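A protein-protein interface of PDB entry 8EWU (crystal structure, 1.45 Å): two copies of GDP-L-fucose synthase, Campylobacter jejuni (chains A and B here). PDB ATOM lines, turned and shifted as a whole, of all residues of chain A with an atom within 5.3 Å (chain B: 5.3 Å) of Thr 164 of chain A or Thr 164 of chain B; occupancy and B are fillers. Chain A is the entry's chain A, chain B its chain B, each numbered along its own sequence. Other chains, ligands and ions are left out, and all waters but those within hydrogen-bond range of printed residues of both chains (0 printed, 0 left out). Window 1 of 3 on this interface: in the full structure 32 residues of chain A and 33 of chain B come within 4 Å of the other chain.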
ATOM      1  N   LEU A 102     -18.245  15.904  21.258  1.00  0.00           N
ATOM      2  CA  LEU A 102     -18.317  14.425  21.093  1.00  0.00           C
ATOM      3  C   LEU A 102     -19.028  13.848  22.317  1.00  0.00           C
ATOM      4  O   LEU A 102     -20.014  13.137  22.169  1.00  0.00           O
ATOM      5  CB  LEU A 102     -16.941  13.796  20.902  1.00  0.00           C
ATOM      6  CG  LEU A 102     -16.970  12.278  20.792  1.00  0.00           C
ATOM      7  CD1 LEU A 102     -17.805  11.800  19.617  1.00  0.00           C
ATOM      8  CD2 LEU A 102     -15.577  11.686  20.756  1.00  0.00           C
ATOM      9  N   LEU A 106     -22.579  11.820  22.360  1.00  0.00           N
ATOM     10  CA  LEU A 106     -22.371  10.338  22.412  1.00  0.00           C
ATOM     11  C   LEU A 106     -23.226   9.738  23.531  1.00  0.00           C
ATOM     12  O   LEU A 106     -23.957   8.763  23.301  1.00  0.00           O
ATOM     13  CB  LEU A 106     -20.907   9.981  22.717  1.00  0.00           C
ATOM     14  CG  LEU A 106     -19.982   9.697  21.545  1.00  0.00           C
ATOM     15  CD1 LEU A 106     -18.630   9.229  22.050  1.00  0.00           C
ATOM     16  CD2 LEU A 106     -20.572   8.655  20.600  1.00  0.00           C
ATOM     17  N   GLN A 109     -27.274  10.208  23.241  1.00  0.00           N
ATOM     18  CA  GLN A 109     -27.902   9.351  22.226  1.00  0.00           C
ATOM     19  C   GLN A 109     -27.739   7.884  22.621  1.00  0.00           C
ATOM     20  O   GLN A 109     -28.634   7.057  22.347  1.00  0.00           O
ATOM     21  CB  GLN A 109     -27.334   9.611  20.832  1.00  0.00           C
ATOM     22  CG  GLN A 109     -25.944   9.037  20.615  1.00  0.00           C
ATOM     23  CD  GLN A 109     -25.227   9.593  19.403  1.00  0.00           C
ATOM     24  OE1 GLN A 109     -25.587  10.684  18.912  1.00  0.00           O
ATOM     25  NE2 GLN A 109     -24.186   8.882  18.932  1.00  0.00           N
ATOM     26  N   ALA A 159     -19.531  15.288  14.102  1.00  0.00           N
ATOM     27  CA  ALA A 159     -19.606  14.319  12.989  1.00  0.00           C
ATOM     28  C   ALA A 159     -19.418  12.887  13.514  1.00  0.00           C
ATOM     29  O   ALA A 159     -20.147  11.944  13.090  1.00  0.00           O
ATOM     30  CB  ALA A 159     -18.595  14.573  11.938  1.00  0.00           C
ATOM     31  N   VAL A 160     -18.438  12.686  14.387  1.00  0.00           N
ATOM     32  CA  VAL A 160     -18.137  11.335  14.938  1.00  0.00           C
ATOM     33  C   VAL A 160     -19.296  10.906  15.825  1.00  0.00           C
ATOM     34  O   VAL A 160     -19.712   9.763  15.703  1.00  0.00           O
ATOM     35  CB  VAL A 160     -16.801  11.303  15.690  1.00  0.00           C
ATOM     36  CG1 VAL A 160     -16.622  10.022  16.486  1.00  0.00           C
ATOM     37  CG2 VAL A 160     -15.682  11.495  14.704  1.00  0.00           C
ATOM     38  N   ALA A 161     -19.862  11.794  16.629  1.00  0.00           N
ATOM     39  CA  ALA A 161     -21.041  11.450  17.443  1.00  0.00           C
ATOM     40  C   ALA A 161     -22.176  10.999  16.511  1.00  0.00           C
ATOM     41  O   ALA A 161     -22.821   9.926  16.749  1.00  0.00           O
ATOM     42  CB  ALA A 161     -21.445  12.608  18.318  1.00  0.00           C
ATOM     43  N   LYS A 162     -22.376  11.729  15.434  1.00  0.00           N
ATOM     44  CA  LYS A 162     -23.528  11.456  14.532  1.00  0.00           C
ATOM     45  C   LYS A 162     -23.297  10.190  13.730  1.00  0.00           C
ATOM     46  O   LYS A 162     -24.245   9.381  13.519  1.00  0.00           O
ATOM     47  CB  LYS A 162     -23.840  12.660  13.645  1.00  0.00           C
ATOM     48  CG  LYS A 162     -24.401  13.839  14.418  1.00  0.00           C
ATOM     49  CD  LYS A 162     -25.585  13.470  15.285  1.00  0.00           C
ATOM     50  CE  LYS A 162     -26.486  14.627  15.601  1.00  0.00           C
ATOM     51  NZ  LYS A 162     -27.564  14.291  16.535  1.00  0.00           N
ATOM     52  N   ILE A 163     -22.100   9.994  13.198  1.00  0.00           N
ATOM     53  CA  ILE A 163     -21.771   8.719  12.475  1.00  0.00           C
ATOM     54  C   ILE A 163     -22.031   7.544  13.411  1.00  0.00           C
ATOM     55  O   ILE A 163     -22.668   6.527  13.039  1.00  0.00           O
ATOM     56  CB  ILE A 163     -20.321   8.720  11.956  1.00  0.00           C
ATOM     57  CG1 ILE A 163     -20.119   9.709  10.823  1.00  0.00           C
ATOM     58  CG2 ILE A 163     -19.864   7.301  11.565  1.00  0.00           C
ATOM     59  CD1 ILE A 163     -18.678   9.980  10.448  1.00  0.00           C
ATOM     60  N   THR A 164     -21.578   7.650  14.654  1.00  0.00           N
ATOM     61  CA  THR A 164     -21.734   6.574  15.648  1.00  0.00           C
ATOM     62  C   THR A 164     -23.214   6.339  15.951  1.00  0.00           C
ATOM     63  O   THR A 164     -23.592   5.198  16.009  1.00  0.00           O
ATOM     64  CB  THR A 164     -20.918   6.870  16.912  1.00  0.00           C
ATOM     65  OG1 THR A 164     -19.557   6.915  16.455  1.00  0.00           O
ATOM     66  CG2 THR A 164     -21.080   5.797  17.951  1.00  0.00           C
ATOM     67  N   GLY A 165     -24.010   7.406  16.034  1.00  0.00           N
ATOM     68  CA  GLY A 165     -25.474   7.304  16.266  1.00  0.00           C
ATOM     69  C   GLY A 165     -26.129   6.659  15.060  1.00  0.00           C
ATOM     70  O   GLY A 165     -26.938   5.665  15.206  1.00  0.00           O
ATOM     71  N   ASN A 166     -25.771   7.082  13.849  1.00  0.00           N
ATOM     72  CA  ASN A 166     -26.366   6.473  12.633  1.00  0.00           C
ATOM     73  C   ASN A 166     -26.068   4.964  12.644  1.00  0.00           C
ATOM     74  O   ASN A 166     -26.949   4.104  12.360  1.00  0.00           O
ATOM     75  CB  ASN A 166     -25.782   7.010  11.314  1.00  0.00           C
ATOM     76  CG  ASN A 166     -26.315   8.357  10.867  1.00  0.00           C
ATOM     77  OD1 ASN A 166     -26.470   8.608   9.640  1.00  0.00           O
ATOM     78  ND2 ASN A 166     -26.680   9.190  11.799  1.00  0.00           N
ATOM     79  N   LYS A 167     -24.785   4.619  12.862  1.00  0.00           N
ATOM     80  CA  LYS A 167     -24.363   3.205  12.819  1.00  0.00           C
ATOM     81  C   LYS A 167     -25.022   2.425  13.967  1.00  0.00           C
ATOM     82  O   LYS A 167     -25.473   1.289  13.741  1.00  0.00           O
ATOM     83  CB  LYS A 167     -22.840   3.074  12.823  1.00  0.00           C
ATOM     84  CG  LYS A 167     -22.132   3.620  11.593  1.00  0.00           C
ATOM     85  CD  LYS A 167     -22.614   3.085  10.265  1.00  0.00           C
ATOM     86  CE  LYS A 167     -22.128   1.699   9.955  1.00  0.00           C
ATOM     87  NZ  LYS A 167     -22.525   1.266   8.570  1.00  0.00           N
ATOM     88  N   MET A 168     -25.184   3.039  15.132  1.00  0.00           N
ATOM     89  CA  MET A 168     -25.882   2.367  16.250  1.00  0.00           C
ATOM     90  C   MET A 168     -27.309   1.992  15.851  1.00  0.00           C
ATOM     91  O   MET A 168     -27.743   0.853  16.130  1.00  0.00           O
ATOM     92  CB  MET A 168     -25.933   3.211  17.515  1.00  0.00           C
ATOM     93  CG  MET A 168     -26.544   2.474  18.692  1.00  0.00           C
ATOM     94  SD  MET A 168     -26.397   3.546  20.167  1.00  0.00           S
ATOM     95  CE  MET A 168     -27.228   2.610  21.465  1.00  0.00           C
ATOM     96  N   CYS A 169     -28.018   2.850  15.157  1.00  0.00           N
ATOM     97  CA  CYS A 169     -29.375   2.537  14.693  1.00  0.00           C
ATOM     98  C   CYS A 169     -29.275   1.335  13.773  1.00  0.00           C
ATOM     99  O   CYS A 169     -30.125   0.445  13.934  1.00  0.00           O
ATOM    100  CB  CYS A 169     -30.036   3.715  13.995  1.00  0.00           C
ATOM    101  SG  CYS A 169     -30.390   5.080  15.120  1.00  0.00           S
ATOM    102  N   LEU B 102     -20.711  -2.628  19.350  1.00  0.00           N
ATOM    103  CA  LEU B 102     -20.612  -1.152  19.421  1.00  0.00           C
ATOM    104  C   LEU B 102     -20.923  -0.674  20.829  1.00  0.00           C
ATOM    105  O   LEU B 102     -20.059   0.014  21.427  1.00  0.00           O
ATOM    106  CB  LEU B 102     -21.505  -0.456  18.397  1.00  0.00           C
ATOM    107  CG  LEU B 102     -21.500   1.066  18.545  1.00  0.00           C
ATOM    108  CD1 LEU B 102     -20.135   1.594  18.184  1.00  0.00           C
ATOM    109  CD2 LEU B 102     -22.559   1.684  17.660  1.00  0.00           C
ATOM    110  N   LEU B 106     -18.257   1.216  23.331  1.00  0.00           N
ATOM    111  CA  LEU B 106     -18.433   2.684  23.312  1.00  0.00           C
ATOM    112  C   LEU B 106     -18.610   3.148  24.758  1.00  0.00           C
ATOM    113  O   LEU B 106     -17.943   4.127  25.169  1.00  0.00           O
ATOM    114  CB  LEU B 106     -19.650   3.021  22.459  1.00  0.00           C
ATOM    115  CG  LEU B 106     -19.885   4.467  22.123  1.00  0.00           C
ATOM    116  CD1 LEU B 106     -18.752   4.932  21.240  1.00  0.00           C
ATOM    117  CD2 LEU B 106     -21.201   4.577  21.371  1.00  0.00           C
ATOM    118  N   GLN B 109     -15.300   2.648  27.201  1.00  0.00           N
ATOM    119  CA  GLN B 109     -14.198   3.591  26.914  1.00  0.00           C
ATOM    120  C   GLN B 109     -14.626   5.019  27.217  1.00  0.00           C
ATOM    121  O   GLN B 109     -13.793   5.792  27.669  1.00  0.00           O
ATOM    122  CB  GLN B 109     -13.748   3.481  25.465  1.00  0.00           C
ATOM    123  CG  GLN B 109     -14.704   4.076  24.438  1.00  0.00           C
ATOM    124  CD  GLN B 109     -14.374   3.635  23.035  1.00  0.00           C
ATOM    125  OE1 GLN B 109     -13.750   2.596  22.848  1.00  0.00           O
ATOM    126  NE2 GLN B 109     -14.885   4.380  22.066  1.00  0.00           N
ATOM    127  N   ALA B 159     -15.128  -1.375  14.859  1.00  0.00           N
ATOM    128  CA  ALA B 159     -14.358  -0.341  14.146  1.00  0.00           C
ATOM    129  C   ALA B 159     -14.905   1.039  14.505  1.00  0.00           C
ATOM    130  O   ALA B 159     -14.112   1.997  14.767  1.00  0.00           O
ATOM    131  CB  ALA B 159     -14.460  -0.531  12.681  1.00  0.00           C
ATOM    132  N   VAL B 160     -16.240   1.175  14.489  1.00  0.00           N
ATOM    133  CA  VAL B 160     -16.852   2.485  14.860  1.00  0.00           C
ATOM    134  C   VAL B 160     -16.523   2.792  16.325  1.00  0.00           C
ATOM    135  O   VAL B 160     -16.227   3.983  16.633  1.00  0.00           O
ATOM    136  CB  VAL B 160     -18.355   2.492  14.573  1.00  0.00           C
ATOM    137  CG1 VAL B 160     -19.094   3.645  15.234  1.00  0.00           C
ATOM    138  CG2 VAL B 160     -18.567   2.446  13.059  1.00  0.00           C
ATOM    139  N   ALA B 161     -16.631   1.843  17.242  1.00  0.00           N
ATOM    140  CA  ALA B 161     -16.263   2.092  18.658  1.00  0.00           C
ATOM    141  C   ALA B 161     -14.796   2.549  18.700  1.00  0.00           C
ATOM    142  O   ALA B 161     -14.506   3.581  19.367  1.00  0.00           O
ATOM    143  CB  ALA B 161     -16.448   0.882  19.535  1.00  0.00           C
ATOM    144  N   LYS B 162     -13.905   1.895  17.961  1.00  0.00           N
ATOM    145  CA  LYS B 162     -12.468   2.241  18.056  1.00  0.00           C
ATOM    146  C   LYS B 162     -12.135   3.581  17.413  1.00  0.00           C
ATOM    147  O   LYS B 162     -11.312   4.329  17.971  1.00  0.00           O
ATOM    148  CB  LYS B 162     -11.659   1.115  17.448  1.00  0.00           C
ATOM    149  CG  LYS B 162     -11.649  -0.158  18.304  1.00  0.00           C
ATOM    150  CD  LYS B 162     -11.263   0.099  19.748  1.00  0.00           C
ATOM    151  CE  LYS B 162     -10.901  -1.133  20.519  1.00  0.00           C
ATOM    152  NZ  LYS B 162     -10.583  -0.824  21.916  1.00  0.00           N
ATOM    153  N   ILE B 163     -12.744   3.890  16.283  1.00  0.00           N
ATOM    154  CA  ILE B 163     -12.548   5.220  15.654  1.00  0.00           C
ATOM    155  C   ILE B 163     -13.006   6.292  16.646  1.00  0.00           C
ATOM    156  O   ILE B 163     -12.295   7.279  16.893  1.00  0.00           O
ATOM    157  CB  ILE B 163     -13.314   5.355  14.337  1.00  0.00           C
ATOM    158  CG1 ILE B 163     -12.671   4.456  13.273  1.00  0.00           C
ATOM    159  CG2 ILE B 163     -13.363   6.824  13.943  1.00  0.00           C
ATOM    160  CD1 ILE B 163     -13.504   4.206  12.040  1.00  0.00           C
ATOM    161  N   THR B 164     -14.164   6.084  17.252  1.00  0.00           N
ATOM    162  CA  THR B 164     -14.722   7.077  18.175  1.00  0.00           C
ATOM    163  C   THR B 164     -13.800   7.231  19.393  1.00  0.00           C
ATOM    164  O   THR B 164     -13.582   8.376  19.834  1.00  0.00           O
ATOM    165  CB  THR B 164     -16.152   6.722  18.542  1.00  0.00           C
ATOM    166  OG1 THR B 164     -16.924   6.793  17.341  1.00  0.00           O
ATOM    167  CG2 THR B 164     -16.717   7.648  19.586  1.00  0.00           C
ATOM    168  N   GLY B 165     -13.208   6.151  19.883  1.00  0.00           N
ATOM    169  CA  GLY B 165     -12.232   6.189  20.979  1.00  0.00           C
ATOM    170  C   GLY B 165     -10.971   6.911  20.566  1.00  0.00           C
ATOM    171  O   GLY B 165     -10.484   7.778  21.313  1.00  0.00           O
ATOM    172  N   ASN B 166     -10.414   6.603  19.398  1.00  0.00           N
ATOM    173  CA  ASN B 166      -9.210   7.314  18.908  1.00  0.00           C
ATOM    174  C   ASN B 166      -9.494   8.819  18.868  1.00  0.00           C
ATOM    175  O   ASN B 166      -8.673   9.625  19.356  1.00  0.00           O
ATOM    176  CB  ASN B 166      -8.804   6.871  17.507  1.00  0.00           C
ATOM    177  CG  ASN B 166      -8.036   5.557  17.389  1.00  0.00           C
ATOM    178  OD1 ASN B 166      -7.120   5.389  16.529  1.00  0.00           O
ATOM    179  ND2 ASN B 166      -8.317   4.625  18.247  1.00  0.00           N
ATOM    180  N   LYS B 167     -10.636   9.176  18.278  1.00  0.00           N
ATOM    181  CA  LYS B 167     -11.001  10.616  18.110  1.00  0.00           C
ATOM    182  C   LYS B 167     -11.261  11.231  19.470  1.00  0.00           C
ATOM    183  O   LYS B 167     -10.816  12.364  19.722  1.00  0.00           O
ATOM    184  CB  LYS B 167     -12.159  10.799  17.135  1.00  0.00           C
ATOM    185  CG  LYS B 167     -11.859  10.313  15.734  1.00  0.00           C
ATOM    186  CD  LYS B 167     -10.680  10.976  15.020  1.00  0.00           C
ATOM    187  CE  LYS B 167     -10.911  12.421  14.657  1.00  0.00           C
ATOM    188  NZ  LYS B 167      -9.731  12.987  13.913  1.00  0.00           N
ATOM    189  N   MET B 168     -11.901  10.525  20.384  1.00  0.00           N
ATOM    190  CA  MET B 168     -12.114  11.073  21.740  1.00  0.00           C
ATOM    191  C   MET B 168     -10.773  11.418  22.426  1.00  0.00           C
ATOM    192  O   MET B 168     -10.621  12.550  22.989  1.00  0.00           O
ATOM    193  CB  MET B 168     -12.871  10.084  22.607  1.00  0.00           C
ATOM    194  CG  MET B 168     -13.206  10.654  23.954  1.00  0.00           C
ATOM    195  SD  MET B 168     -14.272   9.547  24.876  1.00  0.00           S
ATOM    196  CE  MET B 168     -14.426  10.482  26.410  1.00  0.00           C
ATOM    197  N   CYS B 169      -9.738  10.632  22.203  1.00  0.00           N
ATOM    198  CA  CYS B 169      -8.429  10.933  22.815  1.00  0.00           C
ATOM    199  C   CYS B 169      -7.889  12.218  22.155  1.00  0.00           C
ATOM    200  O   CYS B 169      -7.396  13.110  22.870  1.00  0.00           O
ATOM    201  CB  CYS B 169      -7.422   9.805  22.604  1.00  0.00           C
ATOM    202  SG  CYS B 169      -7.815   8.284  23.540  1.00  0.00           S
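The side-chain hydroxyl (OG1) of Thr 164 of chain A is in hydrogen-bond range of the side-chain hydroxyl (OG1) of Thr 164 of chain B.
The backbone carbonyl oxygen (O) of Val 160 of chain A lies within hydrogen-bond range of the side-chain hydroxyl (OG1) of Thr 164 of chain A, 2.9 Å away.
O of Val 160 of chain B is in hydrogen-bond range of OG1 of Thr 164 of chain B, at 3.0 Å.
CD2 of Leu 102 of chain A touches O of Thr 164 of chain B, 3.97 Å away.
Leu 102 of chain A touches Met 168 of chain B.
CG2 of Thr 164 of chain B touches CD1 of Leu 106 of chain A, at 3.5 Å.
Val 160 of chain A touches Thr 164 of chain B (CG1 to OG1, 3.4 Å).
Thr 164 of chain A touches Leu 106 of chain B (CG2 to CD2, 3.6 Å).
Val 160 of chain B touches Thr 164 of chain A.
CD2 of Leu 102 of chain B touches CA of Met 168 of chain A, 3.7 Å away.
Printed residues of chain B within 4 Å of Val 160 of chain A: Thr 164.
Of the printed residues of chain B, Thr 164 of chain A touches Leu 106 (3.6 Å), Val 160 (3.5 Å) and Thr 164 (2.8 Å).
Printed residues of chain A within 4 Å of Leu 106 of chain B: Thr 164.
Printed residues of chain A within 4 Å of Thr 164 of chain B: Leu 102 (3.97 Å), Leu 106 (3.5 Å), Val 160 (3.4 Å) and Thr 164 (2.8 Å).
Of the printed residues of chain A, Met 168 of chain B touches Leu 102.
Cys 169 of chain B touches none of the printed residues of chain A.
The nearest printed residue of chain B that does not touch Thr 164 of chain A is Leu 102 of chain B (4.02 Å).
Printed residues of chain A that touch a printed residue of chain B: Leu 102, Leu 106, Val 160, Thr 164 and Met 168.
Hydrophobic or aromatic side chains of chain B within 4 Å of the printed part of chain A: Leu 102, Leu 106, Val 160 and Met 168.
Among the printed residues, no Asp or Glu carboxylate lies within 4 Å of a Lys or Arg side-chain nitrogen of the other chain.
Leu 102 of chain A touches Thr 164 of chain B, but with the chains exchanged Thr 164 of chain A does not touch Leu 102 of chain B (4.02 Å).
Leu 102 of chain A touches Met 168 of chain B, and with the chains exchanged Met 168 of chain A touches Leu 102 of chain B.
Leu 106 of chain A touches Thr 164 of chain B, and with the chains exchanged Thr 164 of chain A touches Leu 106 of chain B.
Thr 164 of chain B touches its own counterpart, Thr 164 of chain A.
Of the 8 pairs that touch across the chains among the printed residues, 7 have their exchanged pair printed and touching as well.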
